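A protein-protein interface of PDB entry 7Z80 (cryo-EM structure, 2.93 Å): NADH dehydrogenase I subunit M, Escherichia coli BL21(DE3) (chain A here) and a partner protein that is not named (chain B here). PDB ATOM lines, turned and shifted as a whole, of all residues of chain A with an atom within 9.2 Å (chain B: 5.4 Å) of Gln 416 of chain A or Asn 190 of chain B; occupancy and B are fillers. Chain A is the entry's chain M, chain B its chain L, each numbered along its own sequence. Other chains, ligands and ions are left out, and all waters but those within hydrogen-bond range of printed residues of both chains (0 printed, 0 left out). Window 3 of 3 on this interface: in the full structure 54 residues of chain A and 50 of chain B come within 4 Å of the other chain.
Hydrophobic or aromatic side chains of chain A that line the printed part of chain B: Leu 411, Phe 412 and Phe 415. Of the 10 printed residues of chain B, 5 touch a printed residue of chain A. Printed residues of chain B that touch a printed residue of chain A: Leu 185, Phe 186, Ile 187, Tyr 189 and Asn 190. Hydrophobic or aromatic side chains of chain B that line the printed part of chain A: Phe 186, Ile 187 and Tyr 189.
Among the printed residues, merely in contact across the chains: Leu 411 of chain A with Phe 186 of chain B (3.5 Å), Phe 412 of chain A with Leu 185 of chain B (3.5 Å), Phe 412 of chain A with Phe 186 of chain B (3.5 Å), Phe 412 of chain A with Tyr 189 of chain B (3.5 Å), Phe 415 of chain A with Phe 186 of chain B (3.7 Å), Phe 415 of chain A with Ile 187 of chain B (3.6 Å), Gln 416 of chain A with Tyr 189 of chain B (3.5 Å), Gln 416 of chain A with Asn 190 of chain B (3.9 Å) and Thr 422 of chain A with Phe 186 of chain B (3.96 Å).
OG1 of Thr 422 of chain A lies within hydrogen-bond range of N of Phe 415 of chain A (2.9 Å). The side-chain hydroxyl of Thr 422 of chain A is in hydrogen-bond range of the backbone carbonyl oxygen of Val 418 of chain A (2.6 Å). OD2 of Asp 72 of chain B sits at hydrogen-bond distance from OH of Tyr 189 of chain B, at 3.0 Å. The side-chain amide nitrogen of Asn 190 of chain B lies within hydrogen-bond range of the side-chain carboxylate of Glu 191 of chain B, 3.3 Å away.
Gln 416 of chain A touches two residues of chain B. Asn 190 of chain B touches one residue of chain A. No residue of chain A comes within 4 Å of Glu 191 of chain B. Of the printed residues of chain A, Phe 186 of chain B touches Leu 411 (3.5 Å), Phe 412 (3.5 Å), Phe 415 (3.7 Å) and Thr 422 (3.96 Å). Of the printed residues of chain A, Tyr 189 of chain B touches Phe 412 (3.5 Å) and Gln 416 (3.5 Å). Val 420 of chain A touches none of the printed residues of chain B. Leu 336 of chain A touches none of the printed residues of chain B. The nearest printed residue of chain B that does not touch Thr 422 of chain A is Ile 187 of chain B (8.2 Å).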
ATOM      1  N   THR A 332      18.388 -20.370   9.601  1.00  0.00           N
ATOM      2  CA  THR A 332      17.150 -20.351  10.368  1.00  0.00           C
ATOM      3  C   THR A 332      15.911 -20.615   9.523  1.00  0.00           C
ATOM      4  O   THR A 332      14.895 -21.054  10.069  1.00  0.00           O
ATOM      5  CB  THR A 332      16.977 -19.007  11.085  1.00  0.00           C
ATOM      6  OG1 THR A 332      17.363 -17.942  10.208  1.00  0.00           O
ATOM      7  CG2 THR A 332      17.831 -18.961  12.338  1.00  0.00           C
ATOM      8  N   GLY A 333      15.974 -20.377   8.218  1.00  0.00           N
ATOM      9  CA  GLY A 333      14.807 -20.545   7.368  1.00  0.00           C
ATOM     10  C   GLY A 333      13.693 -19.557   7.636  1.00  0.00           C
ATOM     11  O   GLY A 333      12.520 -19.949   7.676  1.00  0.00           O
ATOM     12  N   SER A 334      14.030 -18.283   7.817  1.00  0.00           N
ATOM     13  CA  SER A 334      13.059 -17.249   8.140  1.00  0.00           C
ATOM     14  C   SER A 334      13.190 -16.093   7.158  1.00  0.00           C
ATOM     15  O   SER A 334      14.297 -15.751   6.738  1.00  0.00           O
ATOM     16  CB  SER A 334      13.250 -16.747   9.576  1.00  0.00           C
ATOM     17  OG  SER A 334      12.221 -15.849   9.949  1.00  0.00           O
ATOM     18  N   GLN A 335      12.046 -15.514   6.784  1.00  0.00           N
ATOM     19  CA  GLN A 335      12.036 -14.326   5.931  1.00  0.00           C
ATOM     20  C   GLN A 335      12.737 -13.153   6.605  1.00  0.00           C
ATOM     21  O   GLN A 335      13.611 -12.505   6.012  1.00  0.00           O
ATOM     22  CB  GLN A 335      10.592 -13.956   5.595  1.00  0.00           C
ATOM     23  CG  GLN A 335      10.083 -14.473   4.271  1.00  0.00           C
ATOM     24  CD  GLN A 335      10.196 -13.432   3.179  1.00  0.00           C
ATOM     25  OE1 GLN A 335      11.166 -13.414   2.421  1.00  0.00           O
ATOM     26  NE2 GLN A 335       9.195 -12.578   3.074  1.00  0.00           N
ATOM     27  N   LEU A 336      12.363 -12.876   7.857  1.00  0.00           N
ATOM     28  CA  LEU A 336      12.896 -11.726   8.577  1.00  0.00           C
ATOM     29  C   LEU A 336      14.386 -11.882   8.844  1.00  0.00           C
ATOM     30  O   LEU A 336      15.149 -10.918   8.710  1.00  0.00           O
ATOM     31  CB  LEU A 336      12.124 -11.541   9.881  1.00  0.00           C
ATOM     32  CG  LEU A 336      12.364 -10.274  10.694  1.00  0.00           C
ATOM     33  CD1 LEU A 336      12.301  -9.058   9.797  1.00  0.00           C
ATOM     34  CD2 LEU A 336      11.333 -10.179  11.796  1.00  0.00           C
ATOM     35  N   ALA A 337      14.817 -13.094   9.203  1.00  0.00           N
ATOM     36  CA  ALA A 337      16.233 -13.342   9.456  1.00  0.00           C
ATOM     37  C   ALA A 337      17.060 -13.196   8.184  1.00  0.00           C
ATOM     38  O   ALA A 337      18.175 -12.667   8.227  1.00  0.00           O
ATOM     39  CB  ALA A 337      16.421 -14.728  10.066  1.00  0.00           C
ATOM     40  N   PHE A 408      19.150  -6.750  14.362  1.00  0.00           N
ATOM     41  CA  PHE A 408      17.913  -6.957  15.099  1.00  0.00           C
ATOM     42  C   PHE A 408      16.895  -7.759  14.304  1.00  0.00           C
ATOM     43  O   PHE A 408      16.176  -8.568  14.889  1.00  0.00           O
ATOM     44  CB  PHE A 408      17.326  -5.622  15.549  1.00  0.00           C
ATOM     45  CG  PHE A 408      17.609  -5.310  16.988  1.00  0.00           C
ATOM     46  CD1 PHE A 408      18.905  -5.374  17.477  1.00  0.00           C
ATOM     47  CD2 PHE A 408      16.583  -4.998  17.862  1.00  0.00           C
ATOM     48  CE1 PHE A 408      19.175  -5.104  18.800  1.00  0.00           C
ATOM     49  CE2 PHE A 408      16.847  -4.726  19.189  1.00  0.00           C
ATOM     50  CZ  PHE A 408      18.145  -4.781  19.657  1.00  0.00           C
ATOM     51  N   MET A 409      16.813  -7.584  12.980  1.00  0.00           N
ATOM     52  CA  MET A 409      15.925  -8.467  12.225  1.00  0.00           C
ATOM     53  C   MET A 409      16.466  -9.896  12.175  1.00  0.00           C
ATOM     54  O   MET A 409      15.680 -10.857  12.194  1.00  0.00           O
ATOM     55  CB  MET A 409      15.653  -7.909  10.829  1.00  0.00           C
ATOM     56  CG  MET A 409      15.165  -6.464  10.852  1.00  0.00           C
ATOM     57  SD  MET A 409      14.874  -5.652   9.265  1.00  0.00           S
ATOM     58  CE  MET A 409      15.039  -7.009   8.120  1.00  0.00           C
ATOM     59  N   ILE A 410      17.797 -10.053  12.168  1.00  0.00           N
ATOM     60  CA  ILE A 410      18.404 -11.377  12.318  1.00  0.00           C
ATOM     61  C   ILE A 410      17.970 -12.017  13.631  1.00  0.00           C
ATOM     62  O   ILE A 410      17.536 -13.175  13.666  1.00  0.00           O
ATOM     63  CB  ILE A 410      19.939 -11.275  12.237  1.00  0.00           C
ATOM     64  CG1 ILE A 410      20.400 -11.078  10.798  1.00  0.00           C
ATOM     65  CG2 ILE A 410      20.605 -12.504  12.843  1.00  0.00           C
ATOM     66  CD1 ILE A 410      21.880 -10.800  10.676  1.00  0.00           C
ATOM     67  N   LEU A 411      18.056 -11.259  14.725  1.00  0.00           N
ATOM     68  CA  LEU A 411      17.713 -11.798  16.035  1.00  0.00           C
ATOM     69  C   LEU A 411      16.216 -12.044  16.179  1.00  0.00           C
ATOM     70  O   LEU A 411      15.818 -12.998  16.848  1.00  0.00           O
ATOM     71  CB  LEU A 411      18.208 -10.858  17.129  1.00  0.00           C
ATOM     72  CG  LEU A 411      19.719 -10.767  17.328  1.00  0.00           C
ATOM     73  CD1 LEU A 411      20.041  -9.728  18.380  1.00  0.00           C
ATOM     74  CD2 LEU A 411      20.299 -12.117  17.706  1.00  0.00           C
ATOM     75  N   PHE A 412      15.378 -11.209  15.560  1.00  0.00           N
ATOM     76  CA  PHE A 412      13.934 -11.430  15.602  1.00  0.00           C
ATOM     77  C   PHE A 412      13.559 -12.723  14.888  1.00  0.00           C
ATOM     78  O   PHE A 412      12.811 -13.550  15.428  1.00  0.00           O
ATOM     79  CB  PHE A 412      13.202 -10.238  14.979  1.00  0.00           C
ATOM     80  CG  PHE A 412      12.798  -9.176  15.968  1.00  0.00           C
ATOM     81  CD1 PHE A 412      11.841  -9.432  16.932  1.00  0.00           C
ATOM     82  CD2 PHE A 412      13.358  -7.910  15.916  1.00  0.00           C
ATOM     83  CE1 PHE A 412      11.466  -8.450  17.833  1.00  0.00           C
ATOM     84  CE2 PHE A 412      12.992  -6.930  16.814  1.00  0.00           C
ATOM     85  CZ  PHE A 412      12.044  -7.200  17.773  1.00  0.00           C
ATOM     86  N   GLY A 413      14.099 -12.935  13.682  1.00  0.00           N
ATOM     87  CA  GLY A 413      13.837 -14.182  12.977  1.00  0.00           C
ATOM     88  C   GLY A 413      14.404 -15.395  13.694  1.00  0.00           C
ATOM     89  O   GLY A 413      13.761 -16.450  13.763  1.00  0.00           O
ATOM     90  N   SER A 414      15.611 -15.256  14.251  1.00  0.00           N
ATOM     91  CA  SER A 414      16.227 -16.362  14.973  1.00  0.00           C
ATOM     92  C   SER A 414      15.428 -16.726  16.217  1.00  0.00           C
ATOM     93  O   SER A 414      15.160 -17.906  16.455  1.00  0.00           O
ATOM     94  CB  SER A 414      17.670 -16.009  15.334  1.00  0.00           C
ATOM     95  OG  SER A 414      18.376 -15.537  14.201  1.00  0.00           O
ATOM     96  N   PHE A 415      14.997 -15.727  16.996  1.00  0.00           N
ATOM     97  CA  PHE A 415      14.167 -15.989  18.168  1.00  0.00           C
ATOM     98  C   PHE A 415      12.815 -16.563  17.781  1.00  0.00           C
ATOM     99  O   PHE A 415      12.214 -17.308  18.562  1.00  0.00           O
ATOM    100  CB  PHE A 415      13.981 -14.712  18.985  1.00  0.00           C
ATOM    101  CG  PHE A 415      13.632 -14.961  20.425  1.00  0.00           C
ATOM    102  CD1 PHE A 415      12.311 -15.079  20.823  1.00  0.00           C
ATOM    103  CD2 PHE A 415      14.629 -15.090  21.377  1.00  0.00           C
ATOM    104  CE1 PHE A 415      11.992 -15.314  22.142  1.00  0.00           C
ATOM    105  CE2 PHE A 415      14.314 -15.323  22.700  1.00  0.00           C
ATOM    106  CZ  PHE A 415      12.995 -15.436  23.082  1.00  0.00           C
ATOM    107  N   GLN A 416      12.317 -16.225  16.589  1.00  0.00           N
ATOM    108  CA  GLN A 416      11.152 -16.929  16.074  1.00  0.00           C
ATOM    109  C   GLN A 416      11.470 -18.398  15.818  1.00  0.00           C
ATOM    110  O   GLN A 416      10.597 -19.262  15.962  1.00  0.00           O
ATOM    111  CB  GLN A 416      10.645 -16.255  14.801  1.00  0.00           C
ATOM    112  CG  GLN A 416       9.641 -15.147  15.044  1.00  0.00           C
ATOM    113  CD  GLN A 416       8.867 -14.791  13.797  1.00  0.00           C
ATOM    114  OE1 GLN A 416       9.350 -14.977  12.681  1.00  0.00           O
ATOM    115  NE2 GLN A 416       7.660 -14.273  13.977  1.00  0.00           N
ATOM    116  N   VAL A 417      12.711 -18.704  15.451  1.00  0.00           N
ATOM    117  CA  VAL A 417      13.113 -20.084  15.167  1.00  0.00           C
ATOM    118  C   VAL A 417      13.790 -20.744  16.374  1.00  0.00           C
ATOM    119  O   VAL A 417      13.299 -21.749  16.889  1.00  0.00           O
ATOM    120  CB  VAL A 417      14.008 -20.128  13.907  1.00  0.00           C
ATOM    121  CG1 VAL A 417      14.727 -21.461  13.786  1.00  0.00           C
ATOM    122  CG2 VAL A 417      13.177 -19.851  12.668  1.00  0.00           C
ATOM    123  N   VAL A 418      14.922 -20.209  16.841  1.00  0.00           N
ATOM    124  CA  VAL A 418      15.622 -20.730  18.025  1.00  0.00           C
ATOM    125  C   VAL A 418      15.923 -19.623  19.042  1.00  0.00           C
ATOM    126  O   VAL A 418      16.557 -18.608  18.717  1.00  0.00           O
ATOM    127  CB  VAL A 418      16.887 -21.531  17.634  1.00  0.00           C
ATOM    128  CG1 VAL A 418      16.545 -22.695  16.725  1.00  0.00           C
ATOM    129  CG2 VAL A 418      17.897 -20.677  16.875  1.00  0.00           C
ATOM    130  N   PRO A 419      15.456 -19.758  20.286  1.00  0.00           N
ATOM    131  CA  PRO A 419      15.626 -18.666  21.259  1.00  0.00           C
ATOM    132  C   PRO A 419      16.995 -18.598  21.929  1.00  0.00           C
ATOM    133  O   PRO A 419      17.502 -17.500  22.191  1.00  0.00           O
ATOM    134  CB  PRO A 419      14.526 -18.953  22.293  1.00  0.00           C
ATOM    135  CG  PRO A 419      13.638 -20.001  21.666  1.00  0.00           C
ATOM    136  CD  PRO A 419      14.533 -20.788  20.780  1.00  0.00           C
ATOM    137  N   VAL A 420      17.597 -19.755  22.214  1.00  0.00           N
ATOM    138  CA  VAL A 420      18.830 -19.788  23.002  1.00  0.00           C
ATOM    139  C   VAL A 420      19.995 -19.205  22.212  1.00  0.00           C
ATOM    140  O   VAL A 420      20.811 -18.439  22.744  1.00  0.00           O
ATOM    141  CB  VAL A 420      19.124 -21.225  23.465  1.00  0.00           C
ATOM    142  CG1 VAL A 420      20.236 -21.234  24.498  1.00  0.00           C
ATOM    143  CG2 VAL A 420      17.865 -21.868  24.024  1.00  0.00           C
ATOM    144  N   THR A 422      19.680 -17.040  19.916  1.00  0.00           N
ATOM    145  CA  THR A 422      19.386 -15.612  19.851  1.00  0.00           C
ATOM    146  C   THR A 422      19.876 -14.875  21.094  1.00  0.00           C
ATOM    147  O   THR A 422      20.490 -13.803  20.990  1.00  0.00           O
ATOM    148  CB  THR A 422      17.886 -15.406  19.673  1.00  0.00           C
ATOM    149  OG1 THR A 422      17.432 -16.179  18.559  1.00  0.00           O
ATOM    150  CG2 THR A 422      17.573 -13.943  19.442  1.00  0.00           C
ATOM    151  N   GLN A 497      13.719 -18.743   0.666  1.00  0.00           N
ATOM    152  CA  GLN A 497      13.103 -19.240   1.895  1.00  0.00           C
ATOM    153  C   GLN A 497      11.972 -20.220   1.604  1.00  0.00           C
ATOM    154  O   GLN A 497      11.819 -21.221   2.316  1.00  0.00           O
ATOM    155  CB  GLN A 497      12.593 -18.072   2.736  1.00  0.00           C
ATOM    156  CG  GLN A 497      12.152 -18.472   4.131  1.00  0.00           C
ATOM    157  CD  GLN A 497      10.647 -18.573   4.255  1.00  0.00           C
ATOM    158  OE1 GLN A 497       9.909 -18.116   3.385  1.00  0.00           O
ATOM    159  NE2 GLN A 497      10.184 -19.185   5.338  1.00  0.00           N
ATOM    160  N   ASP B  72       4.771  -9.900   7.819  1.00  0.00           N
ATOM    161  CA  ASP B  72       4.027  -9.577   9.030  1.00  0.00           C
ATOM    162  C   ASP B  72       4.764  -8.556   9.886  1.00  0.00           C
ATOM    163  O   ASP B  72       4.125  -7.733  10.552  1.00  0.00           O
ATOM    164  CB  ASP B  72       3.752 -10.861   9.820  1.00  0.00           C
ATOM    165  CG  ASP B  72       3.456 -10.601  11.286  1.00  0.00           C
ATOM    166  OD1 ASP B  72       2.302 -10.248  11.605  1.00  0.00           O
ATOM    167  OD2 ASP B  72       4.375 -10.757  12.118  1.00  0.00           O
ATOM    168  N   LEU B 185      11.570  -7.424  23.730  1.00  0.00           N
ATOM    169  CA  LEU B 185      11.053  -7.119  22.398  1.00  0.00           C
ATOM    170  C   LEU B 185      10.868  -8.382  21.565  1.00  0.00           C
ATOM    171  O   LEU B 185       9.846  -8.537  20.881  1.00  0.00           O
ATOM    172  CB  LEU B 185      11.992  -6.152  21.675  1.00  0.00           C
ATOM    173  CG  LEU B 185      11.676  -4.656  21.676  1.00  0.00           C
ATOM    174  CD1 LEU B 185      11.628  -4.104  23.085  1.00  0.00           C
ATOM    175  CD2 LEU B 185      12.701  -3.905  20.845  1.00  0.00           C
ATOM    176  N   PHE B 186      11.844  -9.297  21.614  1.00  0.00           N
ATOM    177  CA  PHE B 186      11.759 -10.530  20.833  1.00  0.00           C
ATOM    178  C   PHE B 186      10.598 -11.394  21.301  1.00  0.00           C
ATOM    179  O   PHE B 186       9.843 -11.921  20.474  1.00  0.00           O
ATOM    180  CB  PHE B 186      13.060 -11.337  20.916  1.00  0.00           C
ATOM    181  CG  PHE B 186      14.295 -10.586  20.498  1.00  0.00           C
ATOM    182  CD1 PHE B 186      14.234  -9.540  19.591  1.00  0.00           C
ATOM    183  CD2 PHE B 186      15.528 -10.938  21.019  1.00  0.00           C
ATOM    184  CE1 PHE B 186      15.371  -8.854  19.226  1.00  0.00           C
ATOM    185  CE2 PHE B 186      16.668 -10.256  20.654  1.00  0.00           C
ATOM    186  CZ  PHE B 186      16.588  -9.213  19.759  1.00  0.00           C
ATOM    187  N   ILE B 187      10.431 -11.538  22.620  1.00  0.00           N
ATOM    188  CA  ILE B 187       9.335 -12.348  23.146  1.00  0.00           C
ATOM    189  C   ILE B 187       7.987 -11.725  22.796  1.00  0.00           C
ATOM    190  O   ILE B 187       7.055 -12.427  22.379  1.00  0.00           O
ATOM    191  CB  ILE B 187       9.493 -12.546  24.665  1.00  0.00           C
ATOM    192  CG1 ILE B 187      10.747 -13.363  24.969  1.00  0.00           C
ATOM    193  CG2 ILE B 187       8.285 -13.257  25.247  1.00  0.00           C
ATOM    194  CD1 ILE B 187      11.055 -13.474  26.443  1.00  0.00           C
ATOM    195  N   LEU B 188       7.869 -10.400  22.933  1.00  0.00           N
ATOM    196  CA  LEU B 188       6.597  -9.740  22.658  1.00  0.00           C
ATOM    197  C   LEU B 188       6.226  -9.820  21.182  1.00  0.00           C
ATOM    198  O   LEU B 188       5.052 -10.012  20.847  1.00  0.00           O
ATOM    199  CB  LEU B 188       6.651  -8.288  23.128  1.00  0.00           C
ATOM    200  CG  LEU B 188       6.339  -8.104  24.614  1.00  0.00           C
ATOM    201  CD1 LEU B 188       6.555  -6.667  25.041  1.00  0.00           C
ATOM    202  CD2 LEU B 188       4.919  -8.549  24.915  1.00  0.00           C
ATOM    203  N   TYR B 189       7.207  -9.695  20.282  1.00  0.00           N
ATOM    204  CA  TYR B 189       6.896  -9.841  18.864  1.00  0.00           C
ATOM    205  C   TYR B 189       6.585 -11.289  18.504  1.00  0.00           C
ATOM    206  O   TYR B 189       5.727 -11.549  17.653  1.00  0.00           O
ATOM    207  CB  TYR B 189       8.041  -9.322  17.999  1.00  0.00           C
ATOM    208  CG  TYR B 189       7.875  -9.685  16.541  1.00  0.00           C
ATOM    209  CD1 TYR B 189       6.845  -9.142  15.786  1.00  0.00           C
ATOM    210  CD2 TYR B 189       8.725 -10.597  15.930  1.00  0.00           C
ATOM    211  CE1 TYR B 189       6.676  -9.482  14.460  1.00  0.00           C
ATOM    212  CE2 TYR B 189       8.565 -10.942  14.604  1.00  0.00           C
ATOM    213  CZ  TYR B 189       7.539 -10.381  13.875  1.00  0.00           C
ATOM    214  OH  TYR B 189       7.377 -10.722  12.552  1.00  0.00           O
ATOM    215  N   ASN B 190       7.277 -12.245  19.130  1.00  0.00           N
ATOM    216  CA  ASN B 190       7.028 -13.651  18.828  1.00  0.00           C
ATOM    217  C   ASN B 190       5.638 -14.080  19.278  1.00  0.00           C
ATOM    218  O   ASN B 190       4.979 -14.873  18.596  1.00  0.00           O
ATOM    219  CB  ASN B 190       8.098 -14.524  19.481  1.00  0.00           C
ATOM    220  CG  ASN B 190       7.910 -15.995  19.181  1.00  0.00           C
ATOM    221  OD1 ASN B 190       7.494 -16.370  18.085  1.00  0.00           O
ATOM    222  ND2 ASN B 190       8.215 -16.841  20.158  1.00  0.00           N
ATOM    223  N   GLU B 191       5.170 -13.564  20.413  1.00  0.00           N
ATOM    224  CA  GLU B 191       3.848 -13.944  20.903  1.00  0.00           C
ATOM    225  C   GLU B 191       2.736 -13.098  20.283  1.00  0.00           C
ATOM    226  O   GLU B 191       1.850 -13.630  19.608  1.00  0.00           O
ATOM    227  CB  GLU B 191       3.800 -13.852  22.432  1.00  0.00           C
ATOM    228  CG  GLU B 191       4.879 -14.649  23.148  1.00  0.00           C
ATOM    229  CD  GLU B 191       4.828 -16.128  22.833  1.00  0.00           C
ATOM    230  OE1 GLU B 191       3.732 -16.719  22.921  1.00  0.00           O
ATOM    231  OE2 GLU B 191       5.886 -16.700  22.502  1.00  0.00           O
ATOM    232  N   LEU B 192       2.772 -11.782  20.495  1.00  0.00           N
ATOM    233  CA  LEU B 192       1.659 -10.926  20.106  1.00  0.00           C
ATOM    234  C   LEU B 192       1.692 -10.502  18.645  1.00  0.00           C
ATOM    235  O   LEU B 192       0.637 -10.181  18.087  1.00  0.00           O
ATOM    236  CB  LEU B 192       1.619  -9.683  21.000  1.00  0.00           C
ATOM    237  CG  LEU B 192       1.480 -10.004  22.488  1.00  0.00           C
ATOM    238  CD1 LEU B 192       1.397  -8.740  23.317  1.00  0.00           C
ATOM    239  CD2 LEU B 192       0.256 -10.871  22.717  1.00  0.00           C
ATOM    240  N   GLY B 193       2.861 -10.488  18.012  1.00  0.00           N
ATOM    241  CA  GLY B 193       2.955 -10.136  16.611  1.00  0.00           C
ATOM    242  C   GLY B 193       3.039  -8.657  16.311  1.00  0.00           C
ATOM    243  O   GLY B 193       3.020  -8.281  15.133  1.00  0.00           O
